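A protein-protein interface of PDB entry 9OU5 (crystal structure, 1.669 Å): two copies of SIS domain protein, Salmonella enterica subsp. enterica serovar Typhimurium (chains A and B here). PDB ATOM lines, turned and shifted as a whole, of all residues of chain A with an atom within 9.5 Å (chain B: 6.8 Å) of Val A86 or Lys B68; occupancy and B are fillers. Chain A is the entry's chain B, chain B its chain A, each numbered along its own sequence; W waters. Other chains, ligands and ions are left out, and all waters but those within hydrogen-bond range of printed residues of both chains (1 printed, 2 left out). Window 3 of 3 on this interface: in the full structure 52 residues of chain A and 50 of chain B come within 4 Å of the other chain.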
ATOM      1  N   GLY A  40      16.444  27.601   9.700  1.00  0.00           N
ATOM      2  CA  GLY A  40      17.653  26.785   9.558  1.00  0.00           C
ATOM      3  C   GLY A  40      18.160  26.665   8.116  1.00  0.00           C
ATOM      4  O   GLY A  40      17.524  27.079   7.150  1.00  0.00           O
ATOM      5  N   VAL A  41      19.360  26.112   7.974  1.00  0.00           N
ATOM      6  CA  VAL A  41      19.944  25.830   6.668  1.00  0.00           C
ATOM      7  C   VAL A  41      19.327  24.567   6.076  1.00  0.00           C
ATOM      8  O   VAL A  41      19.421  23.480   6.653  1.00  0.00           O
ATOM      9  CB  VAL A  41      21.468  25.668   6.791  1.00  0.00           C
ATOM     10  CG1 VAL A  41      22.099  25.394   5.415  1.00  0.00           C
ATOM     11  CG2 VAL A  41      22.138  26.856   7.466  1.00  0.00           C
ATOM     12  N   LYS A  42      18.733  24.705   4.889  1.00  0.00           N
ATOM     13  CA  LYS A  42      18.161  23.575   4.170  1.00  0.00           C
ATOM     14  C   LYS A  42      18.793  23.344   2.792  1.00  0.00           C
ATOM     15  O   LYS A  42      18.547  22.309   2.171  1.00  0.00           O
ATOM     16  CB  LYS A  42      16.682  23.857   3.926  1.00  0.00           C
ATOM     17  CG  LYS A  42      15.892  23.968   5.214  1.00  0.00           C
ATOM     18  CD  LYS A  42      14.412  23.711   4.973  1.00  0.00           C
ATOM     19  CE  LYS A  42      13.562  24.159   6.110  1.00  0.00           C
ATOM     20  NZ  LYS A  42      13.636  25.616   6.225  1.00  0.00           N
ATOM     21  N   HIS A  43      19.501  24.341   2.275  1.00  0.00           N
ATOM     22  CA  HIS A  43      19.936  24.341   0.884  1.00  0.00           C
ATOM     23  C   HIS A  43      21.352  24.880   0.844  1.00  0.00           C
ATOM     24  O   HIS A  43      21.624  25.918   1.453  1.00  0.00           O
ATOM     25  CB  HIS A  43      19.076  25.208  -0.063  1.00  0.00           C
ATOM     26  CG  HIS A  43      17.630  24.909  -0.003  1.00  0.00           C
ATOM     27  ND1 HIS A  43      16.761  25.695   0.721  1.00  0.00           N
ATOM     28  CD2 HIS A  43      16.900  23.883  -0.498  1.00  0.00           C
ATOM     29  CE1 HIS A  43      15.535  25.152   0.641  1.00  0.00           C
ATOM     30  NE2 HIS A  43      15.601  24.041  -0.040  1.00  0.00           N
ATOM     31  N   TYR A  45      24.457  25.900  -1.945  1.00  0.00           N
ATOM     32  CA  TYR A  45      24.821  26.165  -3.323  1.00  0.00           C
ATOM     33  C   TYR A  45      26.316  26.448  -3.436  1.00  0.00           C
ATOM     34  O   TYR A  45      26.834  27.291  -2.701  1.00  0.00           O
ATOM     35  CB  TYR A  45      24.080  27.386  -3.881  1.00  0.00           C
ATOM     36  CG  TYR A  45      22.588  27.147  -3.915  1.00  0.00           C
ATOM     37  CD1 TYR A  45      22.062  26.228  -4.795  1.00  0.00           C
ATOM     38  CD2 TYR A  45      21.725  27.761  -3.020  1.00  0.00           C
ATOM     39  CE1 TYR A  45      20.709  25.951  -4.808  1.00  0.00           C
ATOM     40  CE2 TYR A  45      20.361  27.478  -3.000  1.00  0.00           C
ATOM     41  CZ  TYR A  45      19.857  26.566  -3.906  1.00  0.00           C
ATOM     42  OH  TYR A  45      18.529  26.295  -3.966  1.00  0.00           O
ATOM     43  N   ALA A  69      18.646  15.870   4.687  1.00  0.00           N
ATOM     44  CA  ALA A  69      17.795  17.042   4.853  1.00  0.00           C
ATOM     45  C   ALA A  69      18.470  18.321   4.356  1.00  0.00           C
ATOM     46  O   ALA A  69      18.051  19.410   4.714  1.00  0.00           O
ATOM     47  CB  ALA A  69      17.388  17.218   6.318  1.00  0.00           C
ATOM     48  N   LEU A  70      19.541  18.198   3.581  1.00  0.00           N
ATOM     49  CA  LEU A  70      20.165  19.320   2.896  1.00  0.00           C
ATOM     50  C   LEU A  70      20.057  19.075   1.393  1.00  0.00           C
ATOM     51  O   LEU A  70      20.350  17.979   0.927  1.00  0.00           O
ATOM     52  CB  LEU A  70      21.615  19.313   3.355  1.00  0.00           C
ATOM     53  CG  LEU A  70      22.177  20.475   4.171  1.00  0.00           C
ATOM     54  CD1 LEU A  70      21.276  21.298   5.035  1.00  0.00           C
ATOM     55  CD2 LEU A  70      23.318  19.879   4.935  1.00  0.00           C
ATOM     56  N   THR A  71      19.669  20.087   0.624  1.00  0.00           N
ATOM     57  CA  THR A  71      19.837  20.009  -0.811  1.00  0.00           C
ATOM     58  C   THR A  71      21.226  20.561  -1.145  1.00  0.00           C
ATOM     59  O   THR A  71      21.769  21.372  -0.385  1.00  0.00           O
ATOM     60  CB  THR A  71      18.735  20.746  -1.580  1.00  0.00           C
ATOM     61  OG1 THR A  71      18.908  22.151  -1.461  1.00  0.00           O
ATOM     62  CG2 THR A  71      17.316  20.362  -1.210  1.00  0.00           C
ATOM     63  N   TYR A  75      26.683  25.172  -9.406  1.00  0.00           N
ATOM     64  CA  TYR A  75      26.308  26.045 -10.505  1.00  0.00           C
ATOM     65  C   TYR A  75      27.513  26.786 -11.025  1.00  0.00           C
ATOM     66  O   TYR A  75      28.361  27.222 -10.236  1.00  0.00           O
ATOM     67  CB  TYR A  75      25.347  27.183 -10.139  1.00  0.00           C
ATOM     68  CG  TYR A  75      23.905  26.815  -9.913  1.00  0.00           C
ATOM     69  CD1 TYR A  75      23.488  26.213  -8.734  1.00  0.00           C
ATOM     70  CD2 TYR A  75      22.938  27.246 -10.814  1.00  0.00           C
ATOM     71  CE1 TYR A  75      22.151  25.940  -8.505  1.00  0.00           C
ATOM     72  CE2 TYR A  75      21.596  27.025 -10.576  1.00  0.00           C
ATOM     73  CZ  TYR A  75      21.204  26.330  -9.436  1.00  0.00           C
ATOM     74  OH  TYR A  75      19.865  26.121  -9.267  1.00  0.00           O
ATOM     75  N   PHE A  80      23.886  30.775 -12.575  1.00  0.00           N
ATOM     76  CA  PHE A  80      23.242  31.083 -11.310  1.00  0.00           C
ATOM     77  C   PHE A  80      22.657  32.501 -11.280  1.00  0.00           C
ATOM     78  O   PHE A  80      21.543  32.727 -10.815  1.00  0.00           O
ATOM     79  CB  PHE A  80      24.308  30.894 -10.245  1.00  0.00           C
ATOM     80  CG  PHE A  80      23.828  31.123  -8.823  1.00  0.00           C
ATOM     81  CD1 PHE A  80      23.154  30.133  -8.123  1.00  0.00           C
ATOM     82  CD2 PHE A  80      24.027  32.347  -8.206  1.00  0.00           C
ATOM     83  CE1 PHE A  80      22.742  30.339  -6.818  1.00  0.00           C
ATOM     84  CE2 PHE A  80      23.645  32.537  -6.899  1.00  0.00           C
ATOM     85  CZ  PHE A  80      22.982  31.545  -6.207  1.00  0.00           C
ATOM     86  N   ASN A  83      19.683  32.640 -13.709  1.00  0.00           N
ATOM     87  CA  ASN A  83      18.551  31.767 -13.437  1.00  0.00           C
ATOM     88  C   ASN A  83      18.627  31.208 -12.023  1.00  0.00           C
ATOM     89  O   ASN A  83      18.774  29.983 -11.815  1.00  0.00           O
ATOM     90  CB  ASN A  83      18.507  30.611 -14.420  1.00  0.00           C
ATOM     91  CG  ASN A  83      17.185  29.886 -14.385  1.00  0.00           C
ATOM     92  OD1 ASN A  83      16.138  30.478 -14.078  1.00  0.00           O
ATOM     93  ND2 ASN A  83      17.222  28.625 -14.779  1.00  0.00           N
ATOM     94  N   PRO A  84      18.560  32.081 -10.998  1.00  0.00           N
ATOM     95  CA  PRO A  84      18.755  31.621  -9.638  1.00  0.00           C
ATOM     96  C   PRO A  84      17.616  30.736  -9.161  1.00  0.00           C
ATOM     97  O   PRO A  84      16.470  30.913  -9.548  1.00  0.00           O
ATOM     98  CB  PRO A  84      18.867  32.898  -8.819  1.00  0.00           C
ATOM     99  CG  PRO A  84      18.260  33.960  -9.684  1.00  0.00           C
ATOM    100  CD  PRO A  84      18.400  33.541 -11.096  1.00  0.00           C
ATOM    101  N   PRO A  85      17.908  29.704  -8.354  1.00  0.00           N
ATOM    102  CA  PRO A  85      16.851  28.806  -7.867  1.00  0.00           C
ATOM    103  C   PRO A  85      15.847  29.514  -6.963  1.00  0.00           C
ATOM    104  O   PRO A  85      16.250  30.395  -6.205  1.00  0.00           O
ATOM    105  CB  PRO A  85      17.644  27.752  -7.105  1.00  0.00           C
ATOM    106  CG  PRO A  85      18.942  28.446  -6.722  1.00  0.00           C
ATOM    107  CD  PRO A  85      19.259  29.384  -7.839  1.00  0.00           C
ATOM    108  N   VAL A  86      14.578  29.054  -6.922  1.00  0.00           N
ATOM    109  CA  VAL A  86      13.594  29.755  -6.113  1.00  0.00           C
ATOM    110  C   VAL A  86      13.875  29.503  -4.629  1.00  0.00           C
ATOM    111  O   VAL A  86      13.508  30.338  -3.818  1.00  0.00           O
ATOM    112  CB  VAL A  86      12.123  29.460  -6.440  1.00  0.00           C
ATOM    113  CG1 VAL A  86      11.810  29.713  -7.917  1.00  0.00           C
ATOM    114  CG2 VAL A  86      11.776  28.057  -5.974  1.00  0.00           C
ATOM    115  N   ALA A  87      14.653  28.463  -4.287  1.00  0.00           N
ATOM    116  CA  ALA A  87      15.035  28.187  -2.902  1.00  0.00           C
ATOM    117  C   ALA A  87      16.123  29.120  -2.384  1.00  0.00           C
ATOM    118  O   ALA A  87      16.480  29.004  -1.213  1.00  0.00           O
ATOM    119  CB  ALA A  87      15.469  26.730  -2.733  1.00  0.00           C
ATOM    120  N   LEU A  88      16.706  29.977  -3.238  1.00  0.00           N
ATOM    121  CA  LEU A  88      17.690  30.944  -2.780  1.00  0.00           C
ATOM    122  C   LEU A  88      17.031  31.949  -1.824  1.00  0.00           C
ATOM    123  O   LEU A  88      16.167  32.723  -2.206  1.00  0.00           O
ATOM    124  CB  LEU A  88      18.322  31.672  -3.969  1.00  0.00           C
ATOM    125  CG  LEU A  88      19.432  32.674  -3.615  1.00  0.00           C
ATOM    126  CD1 LEU A  88      20.603  32.044  -2.889  1.00  0.00           C
ATOM    127  CD2 LEU A  88      19.905  33.368  -4.831  1.00  0.00           C
ATOM    128  N   GLY A  89      17.460  31.972  -0.571  1.00  0.00           N
ATOM    129  CA  GLY A  89      16.823  32.820   0.431  1.00  0.00           C
ATOM    130  C   GLY A  89      17.409  32.498   1.797  1.00  0.00           C
ATOM    131  O   GLY A  89      18.515  31.956   1.884  1.00  0.00           O
ATOM    132  N   GLU A  90      16.625  32.724   2.850  1.00  0.00           N
ATOM    133  CA  GLU A  90      17.153  32.677   4.212  1.00  0.00           C
ATOM    134  C   GLU A  90      17.489  31.248   4.681  1.00  0.00           C
ATOM    135  O   GLU A  90      18.172  31.088   5.691  1.00  0.00           O
ATOM    136  CB  GLU A  90      16.179  33.431   5.134  1.00  0.00           C
ATOM    137  CG  GLU A  90      14.824  32.754   5.334  1.00  0.00           C
ATOM    138  CD  GLU A  90      13.818  33.564   6.179  1.00  0.00           C
ATOM    139  OE1 GLU A  90      14.113  34.742   6.523  1.00  0.00           O
ATOM    140  OE2 GLU A  90      12.726  33.021   6.482  1.00  0.00           O
ATOM    141  N   ASN A  91      16.981  30.212   3.991  1.00  0.00           N
ATOM    142  CA  ASN A  91      17.273  28.821   4.285  1.00  0.00           C
ATOM    143  C   ASN A  91      18.359  28.252   3.365  1.00  0.00           C
ATOM    144  O   ASN A  91      18.616  27.053   3.401  1.00  0.00           O
ATOM    145  CB  ASN A  91      16.023  27.970   4.257  1.00  0.00           C
ATOM    146  CG  ASN A  91      14.948  28.582   5.128  1.00  0.00           C
ATOM    147  OD1 ASN A  91      13.929  29.068   4.617  1.00  0.00           O
ATOM    148  ND2 ASN A  91      15.169  28.595   6.433  1.00  0.00           N
ATOM    149  N   ALA A  92      19.114  29.132   2.686  1.00  0.00           N
ATOM    150  CA  ALA A  92      20.185  28.719   1.810  1.00  0.00           C
ATOM    151  C   ALA A  92      21.501  29.301   2.297  1.00  0.00           C
ATOM    152  O   ALA A  92      21.545  30.397   2.843  1.00  0.00           O
ATOM    153  CB  ALA A  92      19.901  29.166   0.369  1.00  0.00           C
ATOM    154  N   HIS A 116      19.039  38.197  -1.361  1.00  0.00           N
ATOM    155  CA  HIS A 116      17.974  37.267  -1.020  1.00  0.00           C
ATOM    156  C   HIS A 116      18.012  36.794   0.429  1.00  0.00           C
ATOM    157  O   HIS A 116      17.151  36.033   0.842  1.00  0.00           O
ATOM    158  CB  HIS A 116      18.042  36.056  -1.958  1.00  0.00           C
ATOM    159  CG  HIS A 116      17.465  36.292  -3.294  1.00  0.00           C
ATOM    160  ND1 HIS A 116      18.131  36.872  -4.353  1.00  0.00           N
ATOM    161  CD2 HIS A 116      16.239  35.970  -3.759  1.00  0.00           C
ATOM    162  CE1 HIS A 116      17.336  36.888  -5.413  1.00  0.00           C
ATOM    163  NE2 HIS A 116      16.187  36.350  -5.079  1.00  0.00           N
ATOM    164  N   LEU B  63      13.577  20.630 -11.108  1.00  0.00           N
ATOM    165  CA  LEU B  63      13.462  20.594  -9.653  1.00  0.00           C
ATOM    166  C   LEU B  63      14.492  21.486  -8.937  1.00  0.00           C
ATOM    167  O   LEU B  63      14.166  22.062  -7.899  1.00  0.00           O
ATOM    168  CB  LEU B  63      13.438  19.169  -9.097  1.00  0.00           C
ATOM    169  CG  LEU B  63      12.261  18.306  -9.570  1.00  0.00           C
ATOM    170  CD1 LEU B  63      12.438  16.874  -9.163  1.00  0.00           C
ATOM    171  CD2 LEU B  63      10.977  18.868  -9.004  1.00  0.00           C
ATOM    172  N   GLU B  64      15.705  21.638  -9.467  1.00  0.00           N
ATOM    173  CA  GLU B  64      16.673  22.569  -8.890  1.00  0.00           C
ATOM    174  C   GLU B  64      16.153  24.010  -8.916  1.00  0.00           C
ATOM    175  O   GLU B  64      16.344  24.758  -7.945  1.00  0.00           O
ATOM    176  CB  GLU B  64      18.034  22.555  -9.606  1.00  0.00           C
ATOM    177  CG  GLU B  64      18.747  21.233  -9.374  1.00  0.00           C
ATOM    178  CD  GLU B  64      20.208  21.227  -9.780  1.00  0.00           C
ATOM    179  OE1 GLU B  64      20.521  22.025 -10.712  1.00  0.00           O
ATOM    180  OE2 GLU B  64      20.981  20.458  -9.122  1.00  0.00           O
ATOM    181  N   LYS B  65      15.536  24.415 -10.036  1.00  0.00           N
ATOM    182  CA  LYS B  65      15.006  25.759 -10.176  1.00  0.00           C
ATOM    183  C   LYS B  65      13.789  25.995  -9.282  1.00  0.00           C
ATOM    184  O   LYS B  65      13.668  27.059  -8.685  1.00  0.00           O
ATOM    185  CB  LYS B  65      14.629  26.020 -11.637  1.00  0.00           C
ATOM    186  CG  LYS B  65      13.943  27.357 -11.902  1.00  0.00           C
ATOM    187  CD  LYS B  65      14.799  28.587 -11.620  1.00  0.00           C
ATOM    188  CE  LYS B  65      13.952  29.839 -11.674  1.00  0.00           C
ATOM    189  NZ  LYS B  65      14.822  30.972 -11.949  1.00  0.00           N
ATOM    190  N   GLU B  66      12.873  25.015  -9.244  1.00  0.00           N
ATOM    191  CA  GLU B  66      11.495  25.254  -8.837  1.00  0.00           C
ATOM    192  C   GLU B  66      11.156  24.742  -7.442  1.00  0.00           C
ATOM    193  O   GLU B  66      10.184  25.233  -6.870  1.00  0.00           O
ATOM    194  CB  GLU B  66      10.503  24.580  -9.781  1.00  0.00           C
ATOM    195  CG  GLU B  66      10.630  24.962 -11.257  1.00  0.00           C
ATOM    196  CD  GLU B  66      10.274  26.383 -11.667  1.00  0.00           C
ATOM    197  OE1 GLU B  66      10.539  26.760 -12.833  1.00  0.00           O
ATOM    198  OE2 GLU B  66       9.767  27.118 -10.806  1.00  0.00           O
ATOM    199  N   ALA B  67      11.910  23.785  -6.888  1.00  0.00           N
ATOM    200  CA  ALA B  67      11.502  23.146  -5.646  1.00  0.00           C
ATOM    201  C   ALA B  67      12.133  23.820  -4.424  1.00  0.00           C
ATOM    202  O   ALA B  67      13.285  24.290  -4.470  1.00  0.00           O
ATOM    203  CB  ALA B  67      11.828  21.675  -5.688  1.00  0.00           C
ATOM    204  N   LYS B  68      11.373  23.805  -3.312  1.00  0.00           N
ATOM    205  CA  LYS B  68      11.896  24.258  -2.028  1.00  0.00           C
ATOM    206  C   LYS B  68      12.000  23.147  -0.977  1.00  0.00           C
ATOM    207  O   LYS B  68      12.663  23.369   0.017  1.00  0.00           O
ATOM    208  CB  LYS B  68      11.085  25.428  -1.467  1.00  0.00           C
ATOM    209  CG  LYS B  68      11.178  26.695  -2.279  1.00  0.00           C
ATOM    210  CD  LYS B  68      10.738  27.976  -1.572  1.00  0.00           C
ATOM    211  CE  LYS B  68       9.262  28.201  -1.476  1.00  0.00           C
ATOM    212  NZ  LYS B  68       8.648  28.552  -2.759  1.00  0.00           N
ATOM    213  N   ALA B  69      11.411  21.967  -1.186  1.00  0.00           N
ATOM    214  CA  ALA B  69      11.421  20.888  -0.200  1.00  0.00           C
ATOM    215  C   ALA B  69      11.480  19.499  -0.843  1.00  0.00           C
ATOM    216  O   ALA B  69      10.963  18.525  -0.294  1.00  0.00           O
ATOM    217  CB  ALA B  69      10.168  20.973   0.621  1.00  0.00           C
ATOM    218  N   LEU B  70      11.949  19.424  -2.074  1.00  0.00           N
ATOM    219  CA  LEU B  70      12.291  18.178  -2.748  1.00  0.00           C
ATOM    220  C   LEU B  70      13.765  18.285  -3.091  1.00  0.00           C
ATOM    221  O   LEU B  70      14.166  19.332  -3.604  1.00  0.00           O
ATOM    222  CB  LEU B  70      11.471  18.095  -4.030  1.00  0.00           C
ATOM    223  CG  LEU B  70      10.456  16.971  -4.211  1.00  0.00           C
ATOM    224  CD1 LEU B  70       9.834  16.387  -2.964  1.00  0.00           C
ATOM    225  CD2 LEU B  70       9.427  17.493  -5.182  1.00  0.00           C
ATOM    226  N   THR B  71      14.552  17.237  -2.817  1.00  0.00           N
ATOM    227  CA  THR B  71      15.889  17.125  -3.375  1.00  0.00           C
ATOM    228  C   THR B  71      15.724  16.448  -4.728  1.00  0.00           C
ATOM    229  O   THR B  71      14.789  15.680  -4.929  1.00  0.00           O
ATOM    230  CB  THR B  71      16.831  16.333  -2.468  1.00  0.00           C
ATOM    231  OG1 THR B  71      16.465  14.959  -2.566  1.00  0.00           O
ATOM    232  CG2 THR B  71      16.784  16.759  -1.010  1.00  0.00           C
ATOM    233  N   LEU B 165       6.268  17.823  -7.934  1.00  0.00           N
ATOM    234  CA  LEU B 165       6.261  19.116  -7.270  1.00  0.00           C
ATOM    235  C   LEU B 165       4.826  19.573  -6.987  1.00  0.00           C
ATOM    236  O   LEU B 165       4.517  20.044  -5.888  1.00  0.00           O
ATOM    237  CB  LEU B 165       6.978  20.170  -8.124  1.00  0.00           C
ATOM    238  CG  LEU B 165       7.177  21.536  -7.477  1.00  0.00           C
ATOM    239  CD1 LEU B 165       8.056  21.428  -6.224  1.00  0.00           C
ATOM    240  CD2 LEU B 165       7.792  22.467  -8.524  1.00  0.00           C
ATOM    241  N   GLU B 169       4.378  20.184  -2.954  1.00  0.00           N
ATOM    242  CA  GLU B 169       4.516  21.560  -2.488  1.00  0.00           C
ATOM    243  C   GLU B 169       3.573  22.488  -3.237  1.00  0.00           C
ATOM    244  O   GLU B 169       3.338  23.586  -2.776  1.00  0.00           O
ATOM    245  CB  GLU B 169       5.856  22.235  -2.833  1.00  0.00           C
ATOM    246  CG  GLU B 169       7.068  21.384  -2.514  1.00  0.00           C
ATOM    247  CD  GLU B 169       8.416  21.987  -2.882  1.00  0.00           C
ATOM    248  OE1 GLU B 169       9.308  21.135  -2.940  1.00  0.00           O
ATOM    249  OE2 GLU B 169       8.598  23.226  -3.079  1.00  0.00           O
HETATM  250  O   HOH W   1      17.744  24.312  -5.595  1.00  0.00           O
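The side-chain amide oxygen (OD1) of Asn A83 sits at hydrogen-bond distance from the side-chain amino group (NZ) of Lys B65 (2.6 Å). NZ of Lys B65 lies within hydrogen-bond range of O of Pro A84 (2.9 Å). O of Lys B65 sits at hydrogen-bond distance from N of Val A86 (2.8 Å). The backbone carbonyl oxygen (O) of Lys B68 sits at hydrogen-bond distance from a ring nitrogen (NE2) of His A43, at 3.0 Å.
The side-chain carboxylate (OE2) of Glu B169 lies within hydrogen-bond range of the backbone NH (N) of Lys B68 (2.8 Å). The backbone NH (N) of Thr A71 sits at hydrogen-bond distance from the backbone carbonyl oxygen (O) of Lys A42, 2.9 Å away. The backbone NH (N) of His A43 sits at hydrogen-bond distance from the backbone carbonyl oxygen (O) of Asn A91.
Thr B71 touches Thr A71. Pro A85 touches Glu B64 (CB to O, 3.4 Å). Pro A85 touches Lys B65. CG2 of Val A86 touches O of Glu B66, at 3.4 Å. Lys B68 touches Val A86 (CG to CG2, 3.98 Å). Ala B67 touches Ala A87 (O to CB, 3.7 Å).
Printed residues of chain B within 4 Å of Val A86: Lys B65, Glu B66 and Lys B68. Ala B67 touches just one residue of chain A: Ala A87 (3.7 Å). Ala B69 touches none of the printed residues of chain A. Of the printed residues of chain B, Asn A83 touches Lys B65 (2.6 Å). Printed residues of chain B within 4 Å of Pro A84: Lys B65. Of the printed residues of chain A, Lys B65 touches Asn A83, Pro A84, Pro A85 and Val A86. Of the printed residues of chain A, Glu B64 touches Pro A85 (3.4 Å). Of the printed residues of chain B, His A43 touches Lys B68 (3.0 Å). The nearest printed residue of chain B that does not touch Val A86 is Ala B67 (4.3 Å).
Of the 11 printed residues of chain B, 6 touch a printed residue of chain A.
Thr B71 touches its own counterpart, Thr A71. 3 positions are printed for both chains. Of the 10 pairs that touch across the chains among the printed residues, 1 has its exchanged pair printed and touching as well.
Water W1 lies within hydrogen-bond range of the side-chain hydroxyl of Tyr A45 and the backbone carbonyl oxygen of Glu B64.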
